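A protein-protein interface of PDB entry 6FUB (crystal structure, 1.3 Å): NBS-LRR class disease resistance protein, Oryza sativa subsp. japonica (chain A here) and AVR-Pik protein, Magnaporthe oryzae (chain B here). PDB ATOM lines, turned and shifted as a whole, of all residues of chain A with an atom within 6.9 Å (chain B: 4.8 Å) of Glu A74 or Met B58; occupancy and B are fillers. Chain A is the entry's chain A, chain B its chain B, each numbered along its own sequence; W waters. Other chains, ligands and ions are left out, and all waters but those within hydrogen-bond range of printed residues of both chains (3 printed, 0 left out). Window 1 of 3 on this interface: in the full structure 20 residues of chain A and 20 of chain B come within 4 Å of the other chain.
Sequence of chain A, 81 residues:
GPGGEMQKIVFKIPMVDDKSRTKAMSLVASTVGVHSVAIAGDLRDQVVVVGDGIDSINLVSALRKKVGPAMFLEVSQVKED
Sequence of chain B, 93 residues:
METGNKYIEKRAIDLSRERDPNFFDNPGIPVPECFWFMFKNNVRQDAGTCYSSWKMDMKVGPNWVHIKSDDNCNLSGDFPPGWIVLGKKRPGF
The backbone carbonyl oxygen (O) of Asp B57 sits at hydrogen-bond distance from the backbone NH (N) of Val A75.
The backbone carbonyl oxygen of Leu A73 is in hydrogen-bond range of the backbone NH of Lys B59, 2.8 Å away.
The backbone NH (N) of Ile B67 sits at hydrogen-bond distance from the backbone carbonyl oxygen (O) of Met B56 (2.8 Å).
The backbone carbonyl oxygen (O) of Met B58 lies within hydrogen-bond range of the backbone NH (N) of Val B65, 2.8 Å away.
The backbone NH of Lys A8 lies within hydrogen-bond range of the backbone carbonyl oxygen of Ser A76, 2.8 Å away.
O of Val A10 lies within hydrogen-bond range of N of Leu A73 (2.8 Å).
N of Val A10 sits at hydrogen-bond distance from O of Glu A74 (2.9 Å).
The side-chain hydroxyl (OG) of Ser A76 lies within hydrogen-bond range of the side-chain carboxylate (OE2) of Glu A74 (2.7 Å).
O of Phe A72 touches CB of Lys B59 (3.4 Å).
Phe A72 touches Trp B64 (CB to CH2, 3.7 Å).
Leu A73 touches Met B38.
Leu A73 touches Met B58.
Met B56 touches Glu A74.
CA of Glu A74 touches O of Asp B57, 3.2 Å away.
OE1 of Glu A74 touches CE of Met B58, at 3.9 Å.
Ser A76 touches Met B56 (CB to CB, 3.7 Å).
Of the printed residues of chain B, Glu A74 touches Met B56, Asp B57 and Met B58.
Of chain A, only Leu A73 and Glu A74 come within 4 Å of Met B58.
Of the printed residues of chain B, Phe A72 touches Lys B59 (3.4 Å) and Trp B64 (3.7 Å).
Of the printed residues of chain A, Asp B57 touches Glu A74 and Val A75.
Printed residues of chain A within 4 Å of Met B56: Glu A74 and Ser A76.
Gln A77 touches none of the printed residues of chain B.
Lys A12 touches none of the printed residues of chain B.
The nearest printed residue of chain B that does not touch Val A75 is Met B56 (4.1 Å).
Hydrophobic or aromatic side chains of chain B that line the printed part of chain A: Met B38, Met B56, Met B58 and Trp B64.
Of the 13 printed residues of chain A, 5 touch a printed residue of chain B.
Printed residues of chain A that touch a printed residue of chain B: Phe A72, Leu A73, Glu A74, Val A75 and Ser A76.
Hydrophobic or aromatic side chains of chain A that line the printed part of chain B: Phe A72 and Leu A73.
Among the printed residues, no Asp or Glu carboxylate lies within 4 Å of a Lys or Arg side-chain nitrogen of the other chain.
Water W1 lies within hydrogen-bond range of the side-chain carboxylate of Glu A74 and the indole nitrogen of Trp B36.
Water W3 bridges the side-chain carboxylate of Asp B57 (2.6 Å) and the backbone carbonyl oxygen of Val A75 (2.9 Å).
Water W2 bridges the backbone carbonyl oxygen of Phe A72 (3.0 Å) and the side-chain amino group of Lys B59 (3.1 Å).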
ATOM      1  N   LYS A   8       4.560  13.443  20.883  1.00  0.00           N
ATOM      2  CA  LYS A   8       5.473  14.325  21.606  1.00  0.00           C
ATOM      3  C   LYS A   8       6.887  13.736  21.456  1.00  0.00           C
ATOM      4  O   LYS A   8       7.156  12.561  21.798  1.00  0.00           O
ATOM      5  CB  LYS A   8       5.107  14.408  23.062  1.00  0.00           C
ATOM      6  CG  LYS A   8       5.943  15.388  23.855  1.00  0.00           C
ATOM      7  CD  LYS A   8       5.489  15.422  25.333  1.00  0.00           C
ATOM      8  CE  LYS A   8       6.323  16.366  26.183  1.00  0.00           C
ATOM      9  NZ  LYS A   8       5.706  16.538  27.551  1.00  0.00           N
ATOM     10  N   ILE A   9       7.792  14.576  20.926  1.00  0.00           N
ATOM     11  CA  ILE A   9       9.179  14.139  20.681  1.00  0.00           C
ATOM     12  C   ILE A   9      10.055  15.198  21.318  1.00  0.00           C
ATOM     13  O   ILE A   9       9.867  16.379  21.024  1.00  0.00           O
ATOM     14  CB  ILE A   9       9.499  14.052  19.186  1.00  0.00           C
ATOM     15  CG1 ILE A   9       8.597  13.003  18.511  1.00  0.00           C
ATOM     16  CG2 ILE A   9      10.960  13.647  18.994  1.00  0.00           C
ATOM     17  CD1 ILE A   9       8.473  13.195  17.023  1.00  0.00           C
ATOM     18  N   VAL A  10      10.920  14.791  22.229  1.00  0.00           N
ATOM     19  CA  VAL A  10      11.820  15.716  22.863  1.00  0.00           C
ATOM     20  C   VAL A  10      13.240  15.349  22.470  1.00  0.00           C
ATOM     21  O   VAL A  10      13.672  14.208  22.610  1.00  0.00           O
ATOM     22  CB  VAL A  10      11.651  15.749  24.384  1.00  0.00           C
ATOM     23  CG1 VAL A  10      12.444  16.914  24.939  1.00  0.00           C
ATOM     24  CG2 VAL A  10      10.167  15.827  24.766  1.00  0.00           C
ATOM     25  N   PHE A  11      13.971  16.342  21.977  1.00  0.00           N
ATOM     26  CA  PHE A  11      15.409  16.239  21.747  1.00  0.00           C
ATOM     27  C   PHE A  11      16.198  17.002  22.786  1.00  0.00           C
ATOM     28  O   PHE A  11      15.723  18.001  23.308  1.00  0.00           O
ATOM     29  CB  PHE A  11      15.798  16.776  20.376  1.00  0.00           C
ATOM     30  CG  PHE A  11      15.101  16.115  19.231  1.00  0.00           C
ATOM     31  CD1 PHE A  11      15.524  14.875  18.737  1.00  0.00           C
ATOM     32  CD2 PHE A  11      13.999  16.696  18.636  1.00  0.00           C
ATOM     33  CE1 PHE A  11      14.882  14.286  17.663  1.00  0.00           C
ATOM     34  CE2 PHE A  11      13.370  16.124  17.548  1.00  0.00           C
ATOM     35  CZ  PHE A  11      13.813  14.902  17.050  1.00  0.00           C
ATOM     36  N   LYS A  12      17.420  16.540  23.005  1.00  0.00           N
ATOM     37  CA  LYS A  12      18.438  17.296  23.647  1.00  0.00           C
ATOM     38  C   LYS A  12      19.438  17.750  22.609  1.00  0.00           C
ATOM     39  O   LYS A  12      19.979  16.910  21.927  1.00  0.00           O
ATOM     40  CB  LYS A  12      19.116  16.507  24.734  1.00  0.00           C
ATOM     41  CG  LYS A  12      18.248  16.294  25.932  1.00  0.00           C
ATOM     42  CD  LYS A  12      18.257  17.446  26.929  1.00  0.00           C
ATOM     43  CE  LYS A  12      19.499  17.297  27.872  1.00  0.00           C
ATOM     44  NZ  LYS A  12      19.712  18.551  28.635  1.00  0.00           N
ATOM     45  N   GLN A  46      16.484  21.594  25.661  1.00  0.00           N
ATOM     46  CA  GLN A  46      15.478  20.562  25.550  1.00  0.00           C
ATOM     47  C   GLN A  46      14.490  21.089  24.528  1.00  0.00           C
ATOM     48  O   GLN A  46      13.849  22.092  24.751  1.00  0.00           O
ATOM     49  CB  GLN A  46      14.898  20.343  26.951  1.00  0.00           C
ATOM     50  CG  GLN A  46      14.132  19.157  27.257  1.00  0.00           C
ATOM     51  CD  GLN A  46      13.549  19.071  28.615  1.00  0.00           C
ATOM     52  OE1 GLN A  46      12.331  19.046  28.712  1.00  0.00           O
ATOM     53  NE2 GLN A  46      14.369  18.953  29.679  1.00  0.00           N
ATOM     54  N   MET A  71      20.247  14.554  20.263  1.00  0.00           N
ATOM     55  CA  MET A  71      19.914  13.235  20.773  1.00  0.00           C
ATOM     56  C   MET A  71      18.461  13.157  21.142  1.00  0.00           C
ATOM     57  O   MET A  71      17.888  14.159  21.570  1.00  0.00           O
ATOM     58  CB  MET A  71      20.777  12.962  21.965  1.00  0.00           C
ATOM     59  CG  MET A  71      22.162  12.711  21.432  1.00  0.00           C
ATOM     60  SD  MET A  71      23.329  12.119  22.608  1.00  0.00           S
ATOM     61  CE  MET A  71      23.432  13.621  23.534  1.00  0.00           C
ATOM     62  N   PHE A  72      17.856  12.007  20.964  1.00  0.00           N
ATOM     63  CA  PHE A  72      16.531  11.790  21.481  1.00  0.00           C
ATOM     64  C   PHE A  72      16.567  11.786  22.998  1.00  0.00           C
ATOM     65  O   PHE A  72      17.422  11.162  23.593  1.00  0.00           O
ATOM     66  CB  PHE A  72      15.952  10.491  20.986  1.00  0.00           C
ATOM     67  CG  PHE A  72      15.504  10.551  19.585  1.00  0.00           C
ATOM     68  CD1 PHE A  72      16.389  10.254  18.526  1.00  0.00           C
ATOM     69  CD2 PHE A  72      14.204  10.856  19.287  1.00  0.00           C
ATOM     70  CE1 PHE A  72      15.937  10.274  17.220  1.00  0.00           C
ATOM     71  CE2 PHE A  72      13.759  10.920  17.979  1.00  0.00           C
ATOM     72  CZ  PHE A  72      14.623  10.615  16.934  1.00  0.00           C
ATOM     73  N   LEU A  73      15.611  12.495  23.613  1.00  0.00           N
ATOM     74  CA  LEU A  73      15.361  12.392  25.039  1.00  0.00           C
ATOM     75  C   LEU A  73      14.067  11.621  25.328  1.00  0.00           C
ATOM     76  O   LEU A  73      14.072  10.812  26.245  1.00  0.00           O
ATOM     77  CB  LEU A  73      15.369  13.763  25.695  1.00  0.00           C
ATOM     78  CG  LEU A  73      14.960  13.822  27.170  1.00  0.00           C
ATOM     79  CD1 LEU A  73      15.905  13.117  28.089  1.00  0.00           C
ATOM     80  CD2 LEU A  73      14.767  15.228  27.659  1.00  0.00           C
ATOM     81  N   GLU A  74      13.023  11.859  24.546  1.00  0.00           N
ATOM     82  CA  GLU A  74      11.734  11.241  24.813  1.00  0.00           C
ATOM     83  C   GLU A  74      10.906  11.103  23.536  1.00  0.00           C
ATOM     84  O   GLU A  74      10.955  11.964  22.651  1.00  0.00           O
ATOM     85  CB  GLU A  74      10.982  12.109  25.811  1.00  0.00           C
ATOM     86  CG  GLU A  74       9.530  11.680  26.106  1.00  0.00           C
ATOM     87  CD  GLU A  74       8.774  12.687  26.913  1.00  0.00           C
ATOM     88  OE1 GLU A  74       9.459  13.495  27.542  1.00  0.00           O
ATOM     89  OE2 GLU A  74       7.520  12.602  26.886  1.00  0.00           O
ATOM     90  N   VAL A  75      10.138  10.017  23.493  1.00  0.00           N
ATOM     91  CA  VAL A  75       9.099   9.802  22.505  1.00  0.00           C
ATOM     92  C   VAL A  75       7.886   9.342  23.296  1.00  0.00           C
ATOM     93  O   VAL A  75       7.970   8.358  24.052  1.00  0.00           O
ATOM     94  CB  VAL A  75       9.502   8.737  21.484  1.00  0.00           C
ATOM     95  CG1 VAL A  75       8.391   8.536  20.477  1.00  0.00           C
ATOM     96  CG2 VAL A  75      10.814   9.118  20.832  1.00  0.00           C
ATOM     97  N   SER A  76       6.768  10.038  23.110  1.00  0.00           N
ATOM     98  CA  SER A  76       5.556   9.665  23.783  1.00  0.00           C
ATOM     99  C   SER A  76       4.362  10.190  23.032  1.00  0.00           C
ATOM    100  O   SER A  76       4.493  10.871  22.037  1.00  0.00           O
ATOM    101  CB  SER A  76       5.602  10.176  25.208  1.00  0.00           C
ATOM    102  OG  SER A  76       5.655  11.611  25.278  1.00  0.00           O
ATOM    103  N   GLN A  77       3.185   9.825  23.537  1.00  0.00           N
ATOM    104  CA  GLN A  77       1.914  10.345  23.066  1.00  0.00           C
ATOM    105  C   GLN A  77       1.352  11.378  24.026  1.00  0.00           C
ATOM    106  O   GLN A  77       1.504  11.229  25.258  1.00  0.00           O
ATOM    107  CB  GLN A  77       0.905   9.209  22.851  1.00  0.00           C
ATOM    108  CG  GLN A  77       1.318   8.203  21.804  1.00  0.00           C
ATOM    109  CD  GLN A  77       1.194   8.780  20.410  1.00  0.00           C
ATOM    110  OE1 GLN A  77       2.199   9.039  19.739  1.00  0.00           O
ATOM    111  NE2 GLN A  77      -0.060   9.015  19.966  1.00  0.00           N
ATOM    112  N   TRP B  36       9.214  15.915  36.274  1.00  0.00           N
ATOM    113  CA  TRP B  36      10.229  14.860  36.396  1.00  0.00           C
ATOM    114  C   TRP B  36      11.586  15.460  36.510  1.00  0.00           C
ATOM    115  O   TRP B  36      11.875  16.506  35.961  1.00  0.00           O
ATOM    116  CB  TRP B  36      10.206  13.825  35.199  1.00  0.00           C
ATOM    117  CG  TRP B  36      10.468  14.421  33.822  1.00  0.00           C
ATOM    118  CD1 TRP B  36       9.557  14.768  32.887  1.00  0.00           C
ATOM    119  CD2 TRP B  36      11.761  14.686  33.210  1.00  0.00           C
ATOM    120  NE1 TRP B  36      10.151  15.244  31.786  1.00  0.00           N
ATOM    121  CE2 TRP B  36      11.521  15.220  31.969  1.00  0.00           C
ATOM    122  CE3 TRP B  36      13.081  14.544  33.648  1.00  0.00           C
ATOM    123  CZ2 TRP B  36      12.563  15.634  31.119  1.00  0.00           C
ATOM    124  CZ3 TRP B  36      14.106  14.941  32.778  1.00  0.00           C
ATOM    125  CH2 TRP B  36      13.845  15.466  31.580  1.00  0.00           C
ATOM    126  N   MET B  38      15.762  14.105  36.509  1.00  0.00           N
ATOM    127  CA  MET B  38      16.677  12.962  36.157  1.00  0.00           C
ATOM    128  C   MET B  38      17.985  13.206  36.858  1.00  0.00           C
ATOM    129  O   MET B  38      18.564  14.299  36.772  1.00  0.00           O
ATOM    130  CB  MET B  38      16.885  12.947  34.657  1.00  0.00           C
ATOM    131  CG  MET B  38      17.849  11.808  34.213  1.00  0.00           C
ATOM    132  SD  MET B  38      18.171  11.728  32.430  1.00  0.00           S
ATOM    133  CE  MET B  38      16.551  11.607  31.732  1.00  0.00           C
ATOM    134  N   MET B  56       5.848   6.924  28.906  1.00  0.00           N
ATOM    135  CA  MET B  56       6.739   7.563  27.936  1.00  0.00           C
ATOM    136  C   MET B  56       8.002   6.722  27.820  1.00  0.00           C
ATOM    137  O   MET B  56       8.314   6.021  28.752  1.00  0.00           O
ATOM    138  CB  MET B  56       7.094   9.014  28.389  1.00  0.00           C
ATOM    139  CG  MET B  56       7.861   9.113  29.694  1.00  0.00           C
ATOM    140  SD  MET B  56       8.023  10.813  30.211  1.00  0.00           S
ATOM    141  CE  MET B  56       8.555  10.631  31.922  1.00  0.00           C
ATOM    142  N   ASP B  57       8.692   6.858  26.687  1.00  0.00           N
ATOM    143  CA  ASP B  57      10.015   6.280  26.548  1.00  0.00           C
ATOM    144  C   ASP B  57      11.024   7.396  26.655  1.00  0.00           C
ATOM    145  O   ASP B  57      10.848   8.422  25.951  1.00  0.00           O
ATOM    146  CB  ASP B  57      10.100   5.501  25.192  1.00  0.00           C
ATOM    147  CG  ASP B  57       9.161   4.278  25.200  1.00  0.00           C
ATOM    148  OD1 ASP B  57       9.284   3.484  26.144  1.00  0.00           O
ATOM    149  OD2 ASP B  57       8.288   4.200  24.303  1.00  0.00           O
ATOM    150  N   MET B  58      11.975   7.249  27.562  1.00  0.00           N
ATOM    151  CA  MET B  58      12.926   8.350  27.829  1.00  0.00           C
ATOM    152  C   MET B  58      14.321   7.731  27.796  1.00  0.00           C
ATOM    153  O   MET B  58      14.578   6.690  28.388  1.00  0.00           O
ATOM    154  CB  MET B  58      12.570   9.009  29.196  1.00  0.00           C
ATOM    155  CG  MET B  58      13.544  10.093  29.570  1.00  0.00           C
ATOM    156  SD  MET B  58      13.050  11.017  31.030  1.00  0.00           S
ATOM    157  CE  MET B  58      11.762  12.048  30.330  1.00  0.00           C
ATOM    158  N   LYS B  59      15.230   8.478  27.210  1.00  0.00           N
ATOM    159  CA  LYS B  59      16.640   8.102  27.198  1.00  0.00           C
ATOM    160  C   LYS B  59      17.289   8.562  28.483  1.00  0.00           C
ATOM    161  O   LYS B  59      17.295   9.796  28.816  1.00  0.00           O
ATOM    162  CB  LYS B  59      17.333   8.732  26.029  1.00  0.00           C
ATOM    163  CG  LYS B  59      18.786   8.176  25.853  1.00  0.00           C
ATOM    164  CD  LYS B  59      18.845   6.681  25.422  1.00  0.00           C
ATOM    165  CE  LYS B  59      20.228   6.143  25.171  1.00  0.00           C
ATOM    166  NZ  LYS B  59      20.534   6.474  23.759  1.00  0.00           N
ATOM    167  N   VAL B  60      17.737   7.663  29.316  1.00  0.00           N
ATOM    168  CA  VAL B  60      18.307   7.885  30.621  1.00  0.00           C
ATOM    169  C   VAL B  60      19.758   7.479  30.544  1.00  0.00           C
ATOM    170  O   VAL B  60      20.057   6.267  30.539  1.00  0.00           O
ATOM    171  CB  VAL B  60      17.541   7.174  31.726  1.00  0.00           C
ATOM    172  CG1 VAL B  60      18.134   7.432  33.099  1.00  0.00           C
ATOM    173  CG2 VAL B  60      16.062   7.487  31.658  1.00  0.00           C
ATOM    174  N   ASN B  63      20.701   4.199  28.206  1.00  0.00           N
ATOM    175  CA  ASN B  63      19.629   3.216  27.999  1.00  0.00           C
ATOM    176  C   ASN B  63      18.271   3.910  27.854  1.00  0.00           C
ATOM    177  O   ASN B  63      17.949   4.847  28.655  1.00  0.00           O
ATOM    178  CB  ASN B  63      19.522   2.263  29.169  1.00  0.00           C
ATOM    179  CG  ASN B  63      20.787   1.352  29.375  1.00  0.00           C
ATOM    180  OD1 ASN B  63      21.576   1.618  30.366  1.00  0.00           O
ATOM    181  ND2 ASN B  63      21.089   0.399  28.501  1.00  0.00           N
ATOM    182  N   TRP B  64      17.436   3.486  26.920  1.00  0.00           N
ATOM    183  CA  TRP B  64      16.055   3.791  26.878  1.00  0.00           C
ATOM    184  C   TRP B  64      15.402   3.143  28.065  1.00  0.00           C
ATOM    185  O   TRP B  64      15.646   1.955  28.466  1.00  0.00           O
ATOM    186  CB  TRP B  64      15.368   3.333  25.613  1.00  0.00           C
ATOM    187  CG  TRP B  64      15.689   4.130  24.486  1.00  0.00           C
ATOM    188  CD1 TRP B  64      16.684   3.907  23.562  1.00  0.00           C
ATOM    189  CD2 TRP B  64      15.110   5.394  24.176  1.00  0.00           C
ATOM    190  NE1 TRP B  64      16.696   4.951  22.653  1.00  0.00           N
ATOM    191  CE2 TRP B  64      15.760   5.879  23.030  1.00  0.00           C
ATOM    192  CE3 TRP B  64      14.074   6.160  24.747  1.00  0.00           C
ATOM    193  CZ2 TRP B  64      15.402   7.107  22.422  1.00  0.00           C
ATOM    194  CZ3 TRP B  64      13.729   7.359  24.148  1.00  0.00           C
ATOM    195  CH2 TRP B  64      14.398   7.836  23.019  1.00  0.00           C
ATOM    196  N   VAL B  65      14.451   3.906  28.640  1.00  0.00           N
ATOM    197  CA  VAL B  65      13.670   3.427  29.734  1.00  0.00           C
ATOM    198  C   VAL B  65      12.212   3.655  29.473  1.00  0.00           C
ATOM    199  O   VAL B  65      11.832   4.792  29.045  1.00  0.00           O
ATOM    200  CB  VAL B  65      14.088   4.109  31.099  1.00  0.00           C
ATOM    201  CG1 VAL B  65      13.283   3.557  32.253  1.00  0.00           C
ATOM    202  CG2 VAL B  65      15.586   3.996  31.326  1.00  0.00           C
ATOM    203  N   ILE B  67       8.993   4.531  31.045  1.00  0.00           N
ATOM    204  CA  ILE B  67       8.628   5.120  32.352  1.00  0.00           C
ATOM    205  C   ILE B  67       7.129   5.226  32.454  1.00  0.00           C
ATOM    206  O   ILE B  67       6.518   5.886  31.589  1.00  0.00           O
ATOM    207  CB  ILE B  67       9.308   6.474  32.534  1.00  0.00           C
ATOM    208  CG1 ILE B  67      10.832   6.365  32.417  1.00  0.00           C
ATOM    209  CG2 ILE B  67       8.838   7.061  33.887  1.00  0.00           C
ATOM    210  CD1 ILE B  67      11.541   7.676  32.622  1.00  0.00           C
ATOM    211  N   VAL B  85      14.855   8.612  37.520  1.00  0.00           N
ATOM    212  CA  VAL B  85      13.969   9.749  37.166  1.00  0.00           C
ATOM    213  C   VAL B  85      12.888   9.685  38.197  1.00  0.00           C
ATOM    214  O   VAL B  85      12.218   8.726  38.418  1.00  0.00           O
ATOM    215  CB  VAL B  85      13.407   9.655  35.722  1.00  0.00           C
ATOM    216  CG1 VAL B  85      12.525  10.874  35.352  1.00  0.00           C
ATOM    217  CG2 VAL B  85      14.546   9.551  34.739  1.00  0.00           C
HETATM  218  O   HOH W   1       8.941  15.492  29.060  1.00  0.00           O
HETATM  219  O   HOH W   2      19.236   9.040  22.629  1.00  0.00           O
HETATM  220  O   HOH W   3       7.592   5.909  22.512  1.00  0.00           O
